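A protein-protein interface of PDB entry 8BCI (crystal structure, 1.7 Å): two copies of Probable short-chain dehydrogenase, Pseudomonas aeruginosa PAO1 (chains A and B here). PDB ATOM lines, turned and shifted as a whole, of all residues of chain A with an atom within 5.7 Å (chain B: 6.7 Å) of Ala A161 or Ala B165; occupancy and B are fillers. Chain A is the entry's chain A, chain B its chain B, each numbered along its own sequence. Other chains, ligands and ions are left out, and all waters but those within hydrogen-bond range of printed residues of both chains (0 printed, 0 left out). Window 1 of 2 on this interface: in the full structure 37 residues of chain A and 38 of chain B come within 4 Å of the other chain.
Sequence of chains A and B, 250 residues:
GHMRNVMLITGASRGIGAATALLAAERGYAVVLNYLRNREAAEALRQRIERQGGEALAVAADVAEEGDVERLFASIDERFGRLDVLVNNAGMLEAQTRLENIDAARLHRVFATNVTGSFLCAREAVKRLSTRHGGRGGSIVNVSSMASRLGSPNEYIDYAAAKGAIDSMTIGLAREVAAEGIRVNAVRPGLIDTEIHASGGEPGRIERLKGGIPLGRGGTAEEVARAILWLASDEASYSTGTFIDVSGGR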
ATOM      1  N   PHE A 111       5.226  13.109   8.268  1.00  0.00           N
ATOM      2  CA  PHE A 111       4.703  14.276   8.967  1.00  0.00           C
ATOM      3  C   PHE A 111       3.299  14.629   8.535  1.00  0.00           C
ATOM      4  O   PHE A 111       2.520  15.138   9.347  1.00  0.00           O
ATOM      5  CB  PHE A 111       5.669  15.431   8.800  1.00  0.00           C
ATOM      6  CG  PHE A 111       6.716  15.425   9.846  1.00  0.00           C
ATOM      7  CD1 PHE A 111       7.721  14.485   9.815  1.00  0.00           C
ATOM      8  CD2 PHE A 111       6.633  16.287  10.920  1.00  0.00           C
ATOM      9  CE1 PHE A 111       8.660  14.441  10.802  1.00  0.00           C
ATOM     10  CE2 PHE A 111       7.574  16.239  11.920  1.00  0.00           C
ATOM     11  CZ  PHE A 111       8.582  15.324  11.858  1.00  0.00           C
ATOM     12  N   VAL A 115       1.459  14.406  11.947  1.00  0.00           N
ATOM     13  CA  VAL A 115       1.528  15.744  12.535  1.00  0.00           C
ATOM     14  C   VAL A 115       0.492  16.675  11.926  1.00  0.00           C
ATOM     15  O   VAL A 115      -0.372  17.188  12.621  1.00  0.00           O
ATOM     16  CB  VAL A 115       2.945  16.340  12.414  1.00  0.00           C
ATOM     17  CG1 VAL A 115       2.963  17.693  13.129  1.00  0.00           C
ATOM     18  CG2 VAL A 115       3.949  15.400  13.013  1.00  0.00           C
ATOM     19  N   ALA A 147       8.304   6.696  21.407  1.00  0.00           N
ATOM     20  CA  ALA A 147       9.345   7.095  20.461  1.00  0.00           C
ATOM     21  C   ALA A 147       9.746   8.557  20.626  1.00  0.00           C
ATOM     22  O   ALA A 147      10.884   8.917  20.325  1.00  0.00           O
ATOM     23  CB  ALA A 147       8.876   6.853  19.018  1.00  0.00           C
ATOM     24  N   TYR A 156      13.183   4.342  13.135  1.00  0.00           N
ATOM     25  CA  TYR A 156      12.485   5.384  12.386  1.00  0.00           C
ATOM     26  C   TYR A 156      12.542   6.702  13.155  1.00  0.00           C
ATOM     27  O   TYR A 156      11.565   7.147  13.782  1.00  0.00           O
ATOM     28  CB  TYR A 156      11.038   4.982  12.061  1.00  0.00           C
ATOM     29  CG  TYR A 156      10.483   3.968  12.995  1.00  0.00           C
ATOM     30  CD1 TYR A 156      10.226   4.290  14.322  1.00  0.00           C
ATOM     31  CD2 TYR A 156      10.204   2.679  12.567  1.00  0.00           C
ATOM     32  CE1 TYR A 156       9.734   3.355  15.202  1.00  0.00           C
ATOM     33  CE2 TYR A 156       9.718   1.731  13.444  1.00  0.00           C
ATOM     34  CZ  TYR A 156       9.479   2.075  14.755  1.00  0.00           C
ATOM     35  OH  TYR A 156       8.979   1.147  15.648  1.00  0.00           O
ATOM     36  N   ILE A 157      13.694   7.367  13.081  1.00  0.00           N
ATOM     37  CA  ILE A 157      13.823   8.656  13.763  1.00  0.00           C
ATOM     38  C   ILE A 157      12.807   9.657  13.235  1.00  0.00           C
ATOM     39  O   ILE A 157      12.399  10.567  13.970  1.00  0.00           O
ATOM     40  CB  ILE A 157      15.256   9.179  13.629  1.00  0.00           C
ATOM     41  CG1 ILE A 157      16.224   8.266  14.386  1.00  0.00           C
ATOM     42  CG2 ILE A 157      15.373  10.573  14.209  1.00  0.00           C
ATOM     43  CD1 ILE A 157      17.690   8.494  14.019  1.00  0.00           C
ATOM     44  N   ASP A 158      12.347   9.490  11.984  1.00  0.00           N
ATOM     45  CA  ASP A 158      11.334  10.383  11.441  1.00  0.00           C
ATOM     46  C   ASP A 158      10.029  10.258  12.228  1.00  0.00           C
ATOM     47  O   ASP A 158       9.389  11.253  12.552  1.00  0.00           O
ATOM     48  CB  ASP A 158      11.101  10.100   9.948  1.00  0.00           C
ATOM     49  CG  ASP A 158      10.781   8.641   9.638  1.00  0.00           C
ATOM     50  OD1 ASP A 158      11.307   7.732  10.285  1.00  0.00           O
ATOM     51  OD2 ASP A 158       9.989   8.386   8.708  1.00  0.00           O
ATOM     52  N   TYR A 159       9.634   9.032  12.551  1.00  0.00           N
ATOM     53  CA  TYR A 159       8.447   8.818  13.365  1.00  0.00           C
ATOM     54  C   TYR A 159       8.635   9.388  14.771  1.00  0.00           C
ATOM     55  O   TYR A 159       7.706   9.986  15.339  1.00  0.00           O
ATOM     56  CB  TYR A 159       8.167   7.322  13.415  1.00  0.00           C
ATOM     57  CG  TYR A 159       6.997   6.917  14.260  1.00  0.00           C
ATOM     58  CD1 TYR A 159       5.720   6.965  13.759  1.00  0.00           C
ATOM     59  CD2 TYR A 159       7.176   6.470  15.548  1.00  0.00           C
ATOM     60  CE1 TYR A 159       4.658   6.586  14.526  1.00  0.00           C
ATOM     61  CE2 TYR A 159       6.126   6.089  16.315  1.00  0.00           C
ATOM     62  CZ  TYR A 159       4.875   6.139  15.802  1.00  0.00           C
ATOM     63  OH  TYR A 159       3.793   5.764  16.551  1.00  0.00           O
ATOM     64  N   ALA A 160       9.820   9.176  15.366  1.00  0.00           N
ATOM     65  CA  ALA A 160      10.061   9.707  16.708  1.00  0.00           C
ATOM     66  C   ALA A 160       9.911  11.221  16.701  1.00  0.00           C
ATOM     67  O   ALA A 160       9.286  11.817  17.597  1.00  0.00           O
ATOM     68  CB  ALA A 160      11.462   9.320  17.175  1.00  0.00           C
ATOM     69  N   ALA A 161      10.456  11.846  15.661  1.00  0.00           N
ATOM     70  CA  ALA A 161      10.350  13.298  15.529  1.00  0.00           C
ATOM     71  C   ALA A 161       8.906  13.723  15.389  1.00  0.00           C
ATOM     72  O   ALA A 161       8.480  14.730  15.982  1.00  0.00           O
ATOM     73  CB  ALA A 161      11.172  13.766  14.324  1.00  0.00           C
ATOM     74  N   ALA A 162       8.131  12.982  14.581  1.00  0.00           N
ATOM     75  CA  ALA A 162       6.721  13.312  14.434  1.00  0.00           C
ATOM     76  C   ALA A 162       6.029  13.300  15.792  1.00  0.00           C
ATOM     77  O   ALA A 162       5.205  14.172  16.106  1.00  0.00           O
ATOM     78  CB  ALA A 162       6.045  12.303  13.487  1.00  0.00           C
ATOM     79  N   LYS A 163       6.340  12.301  16.608  1.00  0.00           N
ATOM     80  CA  LYS A 163       5.678  12.208  17.903  1.00  0.00           C
ATOM     81  C   LYS A 163       6.226  13.242  18.886  1.00  0.00           C
ATOM     82  O   LYS A 163       5.463  13.772  19.696  1.00  0.00           O
ATOM     83  CB  LYS A 163       5.769  10.781  18.430  1.00  0.00           C
ATOM     84  CG  LYS A 163       5.111   9.725  17.518  1.00  0.00           C
ATOM     85  CD  LYS A 163       3.618  10.009  17.305  1.00  0.00           C
ATOM     86  CE  LYS A 163       2.926   8.889  16.550  1.00  0.00           C
ATOM     87  NZ  LYS A 163       1.459   9.139  16.384  1.00  0.00           N
ATOM     88  N   GLY A 164       7.495  13.634  18.784  1.00  0.00           N
ATOM     89  CA  GLY A 164       7.931  14.781  19.564  1.00  0.00           C
ATOM     90  C   GLY A 164       7.184  16.051  19.198  1.00  0.00           C
ATOM     91  O   GLY A 164       6.871  16.879  20.064  1.00  0.00           O
ATOM     92  N   ALA A 165       6.864  16.220  17.908  1.00  0.00           N
ATOM     93  CA  ALA A 165       6.030  17.345  17.496  1.00  0.00           C
ATOM     94  C   ALA A 165       4.647  17.283  18.165  1.00  0.00           C
ATOM     95  O   ALA A 165       4.118  18.302  18.634  1.00  0.00           O
ATOM     96  CB  ALA A 165       5.888  17.361  15.983  1.00  0.00           C
ATOM     97  N   ILE A 166       4.050  16.078  18.231  1.00  0.00           N
ATOM     98  CA  ILE A 166       2.756  15.939  18.896  1.00  0.00           C
ATOM     99  C   ILE A 166       2.849  16.323  20.367  1.00  0.00           C
ATOM    100  O   ILE A 166       1.947  16.966  20.914  1.00  0.00           O
ATOM    101  CB  ILE A 166       2.217  14.509  18.711  1.00  0.00           C
ATOM    102  CG1 ILE A 166       1.884  14.276  17.253  1.00  0.00           C
ATOM    103  CG2 ILE A 166       1.019  14.299  19.626  1.00  0.00           C
ATOM    104  CD1 ILE A 166       0.792  15.225  16.696  1.00  0.00           C
ATOM    105  N   SER A 168       4.867  18.431  21.826  1.00  0.00           N
ATOM    106  CA  SER A 168       4.933  19.876  21.975  1.00  0.00           C
ATOM    107  C   SER A 168       3.610  20.531  21.630  1.00  0.00           C
ATOM    108  O   SER A 168       3.185  21.503  22.284  1.00  0.00           O
ATOM    109  CB  SER A 168       6.079  20.439  21.132  1.00  0.00           C
ATOM    110  OG  SER A 168       7.322  19.924  21.568  1.00  0.00           O
ATOM    111  N   PHE B 111       7.142  23.133   8.843  1.00  0.00           N
ATOM    112  CA  PHE B 111       7.856  21.875   9.019  1.00  0.00           C
ATOM    113  C   PHE B 111       8.903  21.662   7.940  1.00  0.00           C
ATOM    114  O   PHE B 111       9.946  21.034   8.205  1.00  0.00           O
ATOM    115  CB  PHE B 111       6.857  20.728   9.078  1.00  0.00           C
ATOM    116  CG  PHE B 111       6.427  20.457  10.457  1.00  0.00           C
ATOM    117  CD1 PHE B 111       5.575  21.341  11.096  1.00  0.00           C
ATOM    118  CD2 PHE B 111       6.942  19.394  11.166  1.00  0.00           C
ATOM    119  CE1 PHE B 111       5.204  21.136  12.394  1.00  0.00           C
ATOM    120  CE2 PHE B 111       6.578  19.197  12.485  1.00  0.00           C
ATOM    121  CZ  PHE B 111       5.720  20.069  13.088  1.00  0.00           C
ATOM    122  N   VAL B 115      12.113  21.368  10.084  1.00  0.00           N
ATOM    123  CA  VAL B 115      12.296  19.952  10.408  1.00  0.00           C
ATOM    124  C   VAL B 115      12.893  19.190   9.214  1.00  0.00           C
ATOM    125  O   VAL B 115      13.988  18.598   9.301  1.00  0.00           O
ATOM    126  CB  VAL B 115      10.958  19.315  10.838  1.00  0.00           C
ATOM    127  CG1 VAL B 115      11.169  17.850  11.256  1.00  0.00           C
ATOM    128  CG2 VAL B 115      10.290  20.127  11.975  1.00  0.00           C
ATOM    129  N   PHE B 119      16.600  17.350   8.864  1.00  0.00           N
ATOM    130  CA  PHE B 119      16.799  15.942   8.560  1.00  0.00           C
ATOM    131  C   PHE B 119      17.677  15.754   7.333  1.00  0.00           C
ATOM    132  O   PHE B 119      18.571  14.905   7.325  1.00  0.00           O
ATOM    133  CB  PHE B 119      15.465  15.249   8.303  1.00  0.00           C
ATOM    134  CG  PHE B 119      14.852  14.597   9.509  1.00  0.00           C
ATOM    135  CD1 PHE B 119      14.145  15.349  10.444  1.00  0.00           C
ATOM    136  CD2 PHE B 119      14.917  13.210   9.678  1.00  0.00           C
ATOM    137  CE1 PHE B 119      13.550  14.760  11.537  1.00  0.00           C
ATOM    138  CE2 PHE B 119      14.295  12.602  10.766  1.00  0.00           C
ATOM    139  CZ  PHE B 119      13.615  13.395  11.709  1.00  0.00           C
ATOM    140  N   SER B 148       9.953  24.292  22.187  1.00  0.00           N
ATOM    141  CA  SER B 148       9.637  22.859  22.216  1.00  0.00           C
ATOM    142  C   SER B 148       9.074  22.439  23.574  1.00  0.00           C
ATOM    143  O   SER B 148       8.286  21.501  23.664  1.00  0.00           O
ATOM    144  CB  SER B 148      10.845  22.012  21.891  1.00  0.00           C
ATOM    145  OG  SER B 148      11.814  22.137  22.911  1.00  0.00           O
ATOM    146  N   ALA B 160       6.486  25.524  17.778  1.00  0.00           N
ATOM    147  CA  ALA B 160       6.819  24.708  18.950  1.00  0.00           C
ATOM    148  C   ALA B 160       6.878  23.231  18.602  1.00  0.00           C
ATOM    149  O   ALA B 160       7.800  22.510  18.993  1.00  0.00           O
ATOM    150  CB  ALA B 160       5.806  24.940  20.073  1.00  0.00           C
ATOM    151  N   ALA B 161       5.932  22.771  17.804  1.00  0.00           N
ATOM    152  CA  ALA B 161       5.909  21.380  17.405  1.00  0.00           C
ATOM    153  C   ALA B 161       7.091  21.021  16.512  1.00  0.00           C
ATOM    154  O   ALA B 161       7.704  19.971  16.694  1.00  0.00           O
ATOM    155  CB  ALA B 161       4.584  21.083  16.701  1.00  0.00           C
ATOM    156  N   ALA B 162       7.449  21.902  15.578  1.00  0.00           N
ATOM    157  CA  ALA B 162       8.644  21.707  14.784  1.00  0.00           C
ATOM    158  C   ALA B 162       9.870  21.544  15.663  1.00  0.00           C
ATOM    159  O   ALA B 162      10.728  20.693  15.400  1.00  0.00           O
ATOM    160  CB  ALA B 162       8.820  22.905  13.834  1.00  0.00           C
ATOM    161  N   LYS B 163       9.988  22.347  16.717  1.00  0.00           N
ATOM    162  CA  LYS B 163      11.187  22.214  17.532  1.00  0.00           C
ATOM    163  C   LYS B 163      11.101  20.998  18.464  1.00  0.00           C
ATOM    164  O   LYS B 163      12.119  20.422  18.798  1.00  0.00           O
ATOM    165  CB  LYS B 163      11.426  23.521  18.303  1.00  0.00           C
ATOM    166  CG  LYS B 163      11.587  24.696  17.367  1.00  0.00           C
ATOM    167  CD  LYS B 163      12.811  24.547  16.457  1.00  0.00           C
ATOM    168  CE  LYS B 163      13.145  25.804  15.685  1.00  0.00           C
ATOM    169  NZ  LYS B 163      14.413  25.673  14.924  1.00  0.00           N
ATOM    170  N   GLY B 164       9.903  20.550  18.826  1.00  0.00           N
ATOM    171  CA  GLY B 164       9.791  19.274  19.517  1.00  0.00           C
ATOM    172  C   GLY B 164      10.256  18.134  18.629  1.00  0.00           C
ATOM    173  O   GLY B 164      10.875  17.187  19.081  1.00  0.00           O
ATOM    174  N   ALA B 165       9.980  18.233  17.329  1.00  0.00           N
ATOM    175  CA  ALA B 165      10.482  17.229  16.399  1.00  0.00           C
ATOM    176  C   ALA B 165      12.011  17.243  16.369  1.00  0.00           C
ATOM    177  O   ALA B 165      12.660  16.196  16.326  1.00  0.00           O
ATOM    178  CB  ALA B 165       9.883  17.488  15.017  1.00  0.00           C
ATOM    179  N   ILE B 166      12.608  18.437  16.373  1.00  0.00           N
ATOM    180  CA  ILE B 166      14.063  18.537  16.383  1.00  0.00           C
ATOM    181  C   ILE B 166      14.646  17.913  17.644  1.00  0.00           C
ATOM    182  O   ILE B 166      15.669  17.215  17.601  1.00  0.00           O
ATOM    183  CB  ILE B 166      14.495  20.019  16.262  1.00  0.00           C
ATOM    184  CG1 ILE B 166      14.161  20.566  14.876  1.00  0.00           C
ATOM    185  CG2 ILE B 166      15.985  20.118  16.587  1.00  0.00           C
ATOM    186  CD1 ILE B 166      14.810  19.816  13.701  1.00  0.00           C
ATOM    187  N   ASP B 167      14.021  18.150  18.798  1.00  0.00           N
ATOM    188  CA  ASP B 167      14.584  17.579  20.027  1.00  0.00           C
ATOM    189  C   ASP B 167      14.558  16.059  19.949  1.00  0.00           C
ATOM    190  O   ASP B 167      15.516  15.390  20.350  1.00  0.00           O
ATOM    191  CB  ASP B 167      13.803  18.050  21.267  1.00  0.00           C
ATOM    192  CG  ASP B 167      13.985  19.518  21.582  1.00  0.00           C
ATOM    193  OD1 ASP B 167      14.679  20.214  20.815  1.00  0.00           O
ATOM    194  OD2 ASP B 167      13.408  19.978  22.605  1.00  0.00           O
ATOM    195  N   SER B 168      13.460  15.483  19.437  1.00  0.00           N
ATOM    196  CA  SER B 168      13.370  14.029  19.344  1.00  0.00           C
ATOM    197  C   SER B 168      14.365  13.489  18.331  1.00  0.00           C
ATOM    198  O   SER B 168      14.944  12.410  18.524  1.00  0.00           O
ATOM    199  CB  SER B 168      11.961  13.577  18.995  1.00  0.00           C
ATOM    200  OG  SER B 168      11.052  13.912  20.031  1.00  0.00           O
ATOM    201  N   MET B 169      14.558  14.218  17.227  1.00  0.00           N
ATOM    202  CA  MET B 169      15.555  13.794  16.255  1.00  0.00           C
ATOM    203  C   MET B 169      16.954  13.868  16.842  1.00  0.00           C
ATOM    204  O   MET B 169      17.828  13.051  16.486  1.00  0.00           O
ATOM    205  CB  MET B 169      15.443  14.644  14.980  1.00  0.00           C
ATOM    206  CG  MET B 169      16.449  14.271  13.904  1.00  0.00           C
ATOM    207  SD  MET B 169      18.029  15.169  13.890  1.00  0.00           S
ATOM    208  CE  MET B 169      17.472  16.698  13.142  1.00  0.00           C
ATOM    209  N   THR B 170      17.203  14.875  17.681  1.00  0.00           N
ATOM    210  CA  THR B 170      18.505  14.989  18.328  1.00  0.00           C
ATOM    211  C   THR B 170      18.804  13.745  19.155  1.00  0.00           C
ATOM    212  O   THR B 170      19.889  13.150  19.047  1.00  0.00           O
ATOM    213  CB  THR B 170      18.541  16.235  19.192  1.00  0.00           C
ATOM    214  OG1 THR B 170      18.289  17.402  18.395  1.00  0.00           O
ATOM    215  CG2 THR B 170      19.908  16.379  19.874  1.00  0.00           C
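The side-chain hydroxyl (OG) of Ser A168 is in hydrogen-bond range of the backbone carbonyl oxygen (O) of Ser B148, 2.8 Å away.
The backbone carbonyl oxygen (O) of Gly A164 is in hydrogen-bond range of the side-chain hydroxyl (OG) of Ser A168 (3.4 Å). O of Gly B164 sits at hydrogen-bond distance from OG of Ser B168. The side-chain carboxylate of Asp B167 lies within hydrogen-bond range of the side-chain hydroxyl of Ser B148 (2.7 Å).
Among the printed residues, pairs that only touch across the chains: Phe A111 with Phe B111 (3.1 Å), Phe A111 with Val B115 (3.7 Å), Val A115 with Phe B111 (3.6 Å), Ile A157 with Phe B119 (3.8 Å), Ile A157 with Met B169 (3.8 Å), Asp A158 with Phe B119 (3.8 Å), Ala A160 with Ser B168 (3.5 Å), Ala A161 with Phe B119 (3.6 Å), Ala A161 with Ala B165 (3.2 Å), Ala A161 with Ser B168 (3.8 Å), Gly A164 with Gly B164 (3.8 Å), Gly A164 with Ser B168 (3.3 Å), Ala A165 with Phe B111 (3.97 Å), Ala A165 with Ala B161 (3.2 Å), Ala A165 with Gly B164 (3.96 Å), Ala A165 with Ala B165 (3.8 Å), Ser A168 with Ala B160 (3.4 Å), Ser A168 with Ala B161 (3.8 Å) and Ser A168 with Gly B164 (3.3 Å).
Printed residues of chain B within 4 Å of Asp A158: Phe B119. Of the printed residues of chain B, Ala A160 touches Ser B168 (3.5 Å). Ala A161 touches three residues of chain B. Ile A166 touches none of the printed residues of chain B. Of the printed residues of chain B, Ser A168 touches Ser B148, Ala B160, Ala B161 and Gly B164. The nearest printed residue of chain A that does not touch Ala B165 is Gly A164 (4.01 Å). The nearest printed residue of chain A that does not touch Ser B148 is Gly A164 (6.0 Å).
Of the 15 printed residues of chain B, 10 touch a printed residue of chain A. Hydrophobic or aromatic side chains of chain B that line the printed part of chain A: Phe B111, Val B115, Phe B119, Ala B161, Ala B165 and Met B169. Of the 15 printed residues of chain A, 9 touch a printed residue of chain B. Hydrophobic or aromatic side chains of chain A that line the printed part of chain B: Phe A111, Val A115, Ile A157, Ala A161 and Ala A165. Among the printed residues, no Asp or Glu carboxylate lies within 4 Å of a Lys or Arg side-chain nitrogen of the other chain.
Phe A111 touches its own counterpart, Phe B111. Ala A160 touches Ser B168, and with the chains exchanged Ser A168 touches Ala B160. Gly A164 touches its own counterpart, Gly B164. Ala A165 touches its own counterpart, Ala B165.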
